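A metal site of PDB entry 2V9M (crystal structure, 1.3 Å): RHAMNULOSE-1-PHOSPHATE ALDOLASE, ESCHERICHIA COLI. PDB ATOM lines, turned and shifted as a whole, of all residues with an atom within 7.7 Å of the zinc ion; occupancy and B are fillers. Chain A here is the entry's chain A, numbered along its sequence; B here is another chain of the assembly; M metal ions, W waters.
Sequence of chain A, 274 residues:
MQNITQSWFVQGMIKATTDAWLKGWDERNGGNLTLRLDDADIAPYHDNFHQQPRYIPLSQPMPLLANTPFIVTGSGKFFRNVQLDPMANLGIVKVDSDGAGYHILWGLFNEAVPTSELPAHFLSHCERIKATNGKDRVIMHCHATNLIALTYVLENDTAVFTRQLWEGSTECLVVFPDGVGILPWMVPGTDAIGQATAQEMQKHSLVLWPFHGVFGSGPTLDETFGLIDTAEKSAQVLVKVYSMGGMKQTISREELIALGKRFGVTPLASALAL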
ATOM      1  N   TRP A  25      24.203   0.751  17.565  1.00  0.00           N
ATOM      2  CA  TRP A  25      24.245  -0.609  16.992  1.00  0.00           C
ATOM      3  C   TRP A  25      23.717  -1.661  17.932  1.00  0.00           C
ATOM      4  O   TRP A  25      23.708  -2.839  17.551  1.00  0.00           O
ATOM      5  CB  TRP A  25      25.671  -0.966  16.618  1.00  0.00           C
ATOM      6  CG  TRP A  25      26.342  -0.055  15.614  1.00  0.00           C
ATOM      7  CD1 TRP A  25      25.792   0.843  14.762  1.00  0.00           C
ATOM      8  CD2 TRP A  25      27.753  -0.040  15.333  1.00  0.00           C
ATOM      9  NE1 TRP A  25      26.768   1.450  14.002  1.00  0.00           N
ATOM     10  CE2 TRP A  25      27.987   0.926  14.336  1.00  0.00           C
ATOM     11  CE3 TRP A  25      28.842  -0.726  15.885  1.00  0.00           C
ATOM     12  CZ2 TRP A  25      29.247   1.211  13.857  1.00  0.00           C
ATOM     13  CZ3 TRP A  25      30.102  -0.441  15.405  1.00  0.00           C
ATOM     14  CH2 TRP A  25      30.315   0.516  14.398  1.00  0.00           C
ATOM     15  N   ASP A  26      23.403  -1.329  19.197  1.00  0.00           N
ATOM     16  CA  ASP A  26      23.193  -2.354  20.233  1.00  0.00           C
ATOM     17  C   ASP A  26      22.087  -1.970  21.207  1.00  0.00           C
ATOM     18  O   ASP A  26      22.249  -1.867  22.428  1.00  0.00           O
ATOM     19  CB  ASP A  26      24.517  -2.701  20.926  1.00  0.00           C
ATOM     20  CG  ASP A  26      25.486  -3.372  19.991  1.00  0.00           C
ATOM     21  OD1 ASP A  26      26.346  -2.674  19.423  1.00  0.00           O
ATOM     22  OD2 ASP A  26      25.331  -4.616  19.733  1.00  0.00           O
ATOM     23  N   GLU A  27      20.893  -1.783  20.620  1.00  0.00           N
ATOM     24  CA  GLU A  27      19.673  -1.668  21.413  1.00  0.00           C
ATOM     25  C   GLU A  27      19.503  -2.881  22.310  1.00  0.00           C
ATOM     26  O   GLU A  27      19.845  -4.004  21.911  1.00  0.00           O
ATOM     27  CB  GLU A  27      18.455  -1.518  20.464  1.00  0.00           C
ATOM     28  CG  GLU A  27      18.121  -2.771  19.640  1.00  0.00           C
ATOM     29  CD  GLU A  27      18.916  -2.999  18.372  1.00  0.00           C
ATOM     30  OE1 GLU A  27      18.553  -3.965  17.624  1.00  0.00           O
ATOM     31  OE2 GLU A  27      19.876  -2.266  18.090  1.00  0.00           O
ATOM     32  N   ARG A  28      18.909  -2.655  23.489  1.00  0.00           N
ATOM     33  CA  ARG A  28      18.491  -3.767  24.363  1.00  0.00           C
ATOM     34  C   ARG A  28      19.687  -4.665  24.603  1.00  0.00           C
ATOM     35  O   ARG A  28      20.774  -4.143  24.929  1.00  0.00           O
ATOM     36  CB  ARG A  28      17.244  -4.407  23.737  1.00  0.00           C
ATOM     37  CG  ARG A  28      16.383  -5.223  24.698  1.00  0.00           C
ATOM     38  CD  ARG A  28      15.414  -6.137  23.925  1.00  0.00           C
ATOM     39  NE  ARG A  28      16.097  -7.156  23.164  1.00  0.00           N
ATOM     40  CZ  ARG A  28      16.599  -7.282  21.968  1.00  0.00           C
ATOM     41  NH1 ARG A  28      16.610  -6.415  20.968  1.00  0.00           N
ATOM     42  NH2 ARG A  28      17.214  -8.437  21.594  1.00  0.00           N
ATOM     43  N   ASN A  29      19.518  -5.975  24.452  1.00  0.00           N
ATOM     44  CA  ASN A  29      20.590  -6.957  24.575  1.00  0.00           C
ATOM     45  C   ASN A  29      21.106  -7.408  23.212  1.00  0.00           C
ATOM     46  O   ASN A  29      21.749  -8.462  23.075  1.00  0.00           O
ATOM     47  CB  ASN A  29      20.078  -8.142  25.406  1.00  0.00           C
ATOM     48  CG  ASN A  29      19.034  -8.915  24.625  1.00  0.00           C
ATOM     49  OD1 ASN A  29      18.141  -8.359  24.059  1.00  0.00           O
ATOM     50  ND2 ASN A  29      19.161 -10.253  24.542  1.00  0.00           N
ATOM     51  N   GLY A  30      20.907  -6.601  22.163  1.00  0.00           N
ATOM     52  CA  GLY A  30      21.377  -6.930  20.834  1.00  0.00           C
ATOM     53  C   GLY A  30      22.853  -6.815  20.725  1.00  0.00           C
ATOM     54  O   GLY A  30      23.443  -5.804  21.066  1.00  0.00           O
ATOM     55  N   GLY A  31      23.544  -7.832  20.385  1.00  0.00           N
ATOM     56  CA  GLY A  31      24.962  -7.853  20.185  1.00  0.00           C
ATOM     57  C   GLY A  31      25.659  -8.730  21.172  1.00  0.00           C
ATOM     58  O   GLY A  31      25.136  -9.091  22.239  1.00  0.00           O
ATOM     59  N   ASN A  32      26.860  -9.171  20.852  1.00  0.00           N
ATOM     60  CA  ASN A  32      27.668  -9.977  21.711  1.00  0.00           C
ATOM     61  C   ASN A  32      29.128  -9.802  21.259  1.00  0.00           C
ATOM     62  O   ASN A  32      29.417  -9.583  20.085  1.00  0.00           O
ATOM     63  CB  ASN A  32      27.370 -11.499  21.656  1.00  0.00           C
ATOM     64  CG  ASN A  32      25.968 -11.964  21.591  1.00  0.00           C
ATOM     65  OD1 ASN A  32      25.207 -11.779  20.637  1.00  0.00           O
ATOM     66  ND2 ASN A  32      25.508 -12.500  22.689  1.00  0.00           N
ATOM     67  N   GLU A 117      25.505 -18.015  24.065  1.00  0.00           N
ATOM     68  CA  GLU A 117      25.972 -17.774  22.698  1.00  0.00           C
ATOM     69  C   GLU A 117      27.433 -18.164  22.527  1.00  0.00           C
ATOM     70  O   GLU A 117      28.010 -18.116  21.430  1.00  0.00           O
ATOM     71  CB  GLU A 117      25.774 -16.310  22.311  1.00  0.00           C
ATOM     72  CG  GLU A 117      24.347 -15.918  21.934  1.00  0.00           C
ATOM     73  CD  GLU A 117      23.544 -15.218  23.015  1.00  0.00           C
ATOM     74  OE1 GLU A 117      23.285 -15.948  24.012  1.00  0.00           O
ATOM     75  OE2 GLU A 117      23.122 -14.012  22.977  1.00  0.00           O
ATOM     76  N   HIS A 141      29.493  -9.335  17.301  1.00  0.00           N
ATOM     77  CA  HIS A 141      28.180  -9.272  16.656  1.00  0.00           C
ATOM     78  C   HIS A 141      27.495  -7.980  17.100  1.00  0.00           C
ATOM     79  O   HIS A 141      27.407  -7.681  18.300  1.00  0.00           O
ATOM     80  CB  HIS A 141      27.300 -10.453  16.979  1.00  0.00           C
ATOM     81  CG  HIS A 141      25.862 -10.301  16.601  1.00  0.00           C
ATOM     82  ND1 HIS A 141      25.445 -10.039  15.309  1.00  0.00           N
ATOM     83  CD2 HIS A 141      24.726 -10.402  17.313  1.00  0.00           C
ATOM     84  CE1 HIS A 141      24.120  -9.964  15.290  1.00  0.00           C
ATOM     85  NE2 HIS A 141      23.621 -10.180  16.465  1.00  0.00           N
ATOM     86  N   CYS A 142      26.986  -7.189  16.145  1.00  0.00           N
ATOM     87  CA  CYS A 142      26.184  -6.052  16.487  1.00  0.00           C
ATOM     88  C   CYS A 142      25.121  -5.800  15.406  1.00  0.00           C
ATOM     89  O   CYS A 142      25.155  -6.433  14.342  1.00  0.00           O
ATOM     90  CB  CYS A 142      27.040  -4.829  16.725  1.00  0.00           C
ATOM     91  SG  CYS A 142      27.848  -4.261  15.281  1.00  0.00           S
ATOM     92  N   HIS A 143      24.233  -4.890  15.730  1.00  0.00           N
ATOM     93  CA  HIS A 143      23.095  -4.606  14.847  1.00  0.00           C
ATOM     94  C   HIS A 143      23.405  -3.283  14.102  1.00  0.00           C
ATOM     95  O   HIS A 143      22.775  -2.254  14.326  1.00  0.00           O
ATOM     96  CB  HIS A 143      21.786  -4.582  15.619  1.00  0.00           C
ATOM     97  CG  HIS A 143      21.458  -5.927  16.205  1.00  0.00           C
ATOM     98  ND1 HIS A 143      20.380  -6.103  17.008  1.00  0.00           N
ATOM     99  CD2 HIS A 143      22.049  -7.155  16.128  1.00  0.00           C
ATOM    100  CE1 HIS A 143      20.315  -7.387  17.383  1.00  0.00           C
ATOM    101  NE2 HIS A 143      21.323  -8.059  16.840  1.00  0.00           N
ATOM    102  N   PRO A 188      17.942 -17.135  14.596  1.00  0.00           N
ATOM    103  CA  PRO A 188      19.117 -16.955  15.428  1.00  0.00           C
ATOM    104  C   PRO A 188      19.153 -17.926  16.609  1.00  0.00           C
ATOM    105  O   PRO A 188      18.154 -18.484  17.066  1.00  0.00           O
ATOM    106  CB  PRO A 188      19.039 -15.547  15.946  1.00  0.00           C
ATOM    107  CG  PRO A 188      17.808 -14.949  15.426  1.00  0.00           C
ATOM    108  CD  PRO A 188      17.015 -16.000  14.720  1.00  0.00           C
ATOM    109  N   TRP A 209      24.078 -11.201   8.415  1.00  0.00           N
ATOM    110  CA  TRP A 209      22.821 -11.864   8.671  1.00  0.00           C
ATOM    111  C   TRP A 209      21.697 -10.943   8.193  1.00  0.00           C
ATOM    112  O   TRP A 209      21.412  -9.941   8.849  1.00  0.00           O
ATOM    113  CB  TRP A 209      22.704 -12.140  10.170  1.00  0.00           C
ATOM    114  CG  TRP A 209      23.622 -13.189  10.719  1.00  0.00           C
ATOM    115  CD1 TRP A 209      24.530 -13.981  10.061  1.00  0.00           C
ATOM    116  CD2 TRP A 209      23.680 -13.562  12.097  1.00  0.00           C
ATOM    117  NE1 TRP A 209      25.153 -14.813  10.946  1.00  0.00           N
ATOM    118  CE2 TRP A 209      24.639 -14.576  12.205  1.00  0.00           C
ATOM    119  CE3 TRP A 209      23.008 -13.147  13.252  1.00  0.00           C
ATOM    120  CZ2 TRP A 209      24.968 -15.193  13.379  1.00  0.00           C
ATOM    121  CZ3 TRP A 209      23.316 -13.754  14.447  1.00  0.00           C
ATOM    122  CH2 TRP A 209      24.278 -14.776  14.521  1.00  0.00           C
ATOM    123  N   HIS A 212      19.080  -8.523  10.184  1.00  0.00           N
ATOM    124  CA  HIS A 212      19.520  -8.780  11.565  1.00  0.00           C
ATOM    125  C   HIS A 212      20.807  -8.014  11.822  1.00  0.00           C
ATOM    126  O   HIS A 212      20.784  -7.183  12.753  1.00  0.00           O
ATOM    127  CB  HIS A 212      19.639 -10.292  11.806  1.00  0.00           C
ATOM    128  CG  HIS A 212      20.017 -10.666  13.213  1.00  0.00           C
ATOM    129  ND1 HIS A 212      19.821 -11.908  13.737  1.00  0.00           N
ATOM    130  CD2 HIS A 212      20.571 -10.003  14.279  1.00  0.00           C
ATOM    131  CE1 HIS A 212      20.248 -11.954  14.976  1.00  0.00           C
ATOM    132  NE2 HIS A 212      20.727 -10.783  15.360  1.00  0.00           N
ATOM    133  N   GLY A 213      21.942  -8.337  11.272  1.00  0.00           N
ATOM    134  CA  GLY A 213      23.158  -7.644  11.691  1.00  0.00           C
ATOM    135  C   GLY A 213      24.410  -8.227  11.129  1.00  0.00           C
ATOM    136  O   GLY A 213      24.368  -8.875  10.064  1.00  0.00           O
ATOM    137  N   VAL A 214      25.528  -7.949  11.787  1.00  0.00           N
ATOM    138  CA  VAL A 214      26.859  -8.256  11.265  1.00  0.00           C
ATOM    139  C   VAL A 214      27.658  -9.040  12.299  1.00  0.00           C
ATOM    140  O   VAL A 214      27.402  -8.902  13.507  1.00  0.00           O
ATOM    141  CB  VAL A 214      27.587  -6.968  10.807  1.00  0.00           C
ATOM    142  CG1 VAL A 214      27.929  -6.065  11.988  1.00  0.00           C
ATOM    143  CG2 VAL A 214      28.850  -7.267   9.989  1.00  0.00           C
ATOM    144  N   THR B 170      15.137  -8.556  13.105  1.00  0.00           N
ATOM    145  CA  THR B 170      14.738  -9.943  13.401  1.00  0.00           C
ATOM    146  C   THR B 170      14.218 -10.153  14.806  1.00  0.00           C
ATOM    147  O   THR B 170      13.268 -10.902  15.028  1.00  0.00           O
ATOM    148  CB  THR B 170      15.931 -10.884  13.096  1.00  0.00           C
ATOM    149  OG1 THR B 170      16.082 -11.015  11.681  1.00  0.00           O
ATOM    150  CG2 THR B 170      15.701 -12.278  13.655  1.00  0.00           C
ATOM    151  N   GLU B 171      14.827  -9.489  15.796  1.00  0.00           N
ATOM    152  CA  GLU B 171      14.501  -9.569  17.216  1.00  0.00           C
ATOM    153  C   GLU B 171      13.088  -9.133  17.540  1.00  0.00           C
ATOM    154  O   GLU B 171      12.551  -9.521  18.572  1.00  0.00           O
ATOM    155  CB  GLU B 171      15.452  -8.678  18.059  1.00  0.00           C
ATOM    156  CG  GLU B 171      15.322  -7.218  17.670  1.00  0.00           C
ATOM    157  CD  GLU B 171      16.480  -6.309  17.970  1.00  0.00           C
ATOM    158  OE1 GLU B 171      17.425  -6.672  18.647  1.00  0.00           O
ATOM    159  OE2 GLU B 171      16.485  -5.187  17.520  1.00  0.00           O
HETATM  160 ZN    ZN M   1      21.645 -10.078  16.990  1.00  0.00          ZN
HETATM  161  O   HOH W   1      21.787 -10.298  19.108  1.00  0.00           O
HETATM  162  O   HOH W   2      21.530 -12.375  17.702  1.00  0.00           O
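A ring nitrogen (ND1) of His 143 is in hydrogen-bond range of the side-chain carboxylate (OE1) of Glu 27 (2.9 Å).
O of Asn 32 is in hydrogen-bond range of N of His 141, 2.8 Å away.
O of Trp 25 sits at hydrogen-bond distance from N of His 143.
A ring nitrogen (ND1) of His 141 is in hydrogen-bond range of the backbone carbonyl oxygen (O) of Val 214, 2.9 Å away.
The side-chain carboxylate of Glu 171 of chain B sits close to a ring nitrogen (ND1) of His 143, 3.4 Å away.
Within 4 Å of the zinc ion: His 141, His 143 and His 212.
The nearest printed residue that does not touch the zinc ion is Gly 31 (4.5 Å).
NE2 of His 212 binds the zinc ion, at 2.0 Å.
NE2 of His 141 is bound to the zinc ion, at 2.0 Å.
NE2 of His 143 is bound to the zinc ion (2.1 Å).
Water W1 binds the zinc ion.
Water W2 binds the zinc ion (2.4 Å).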
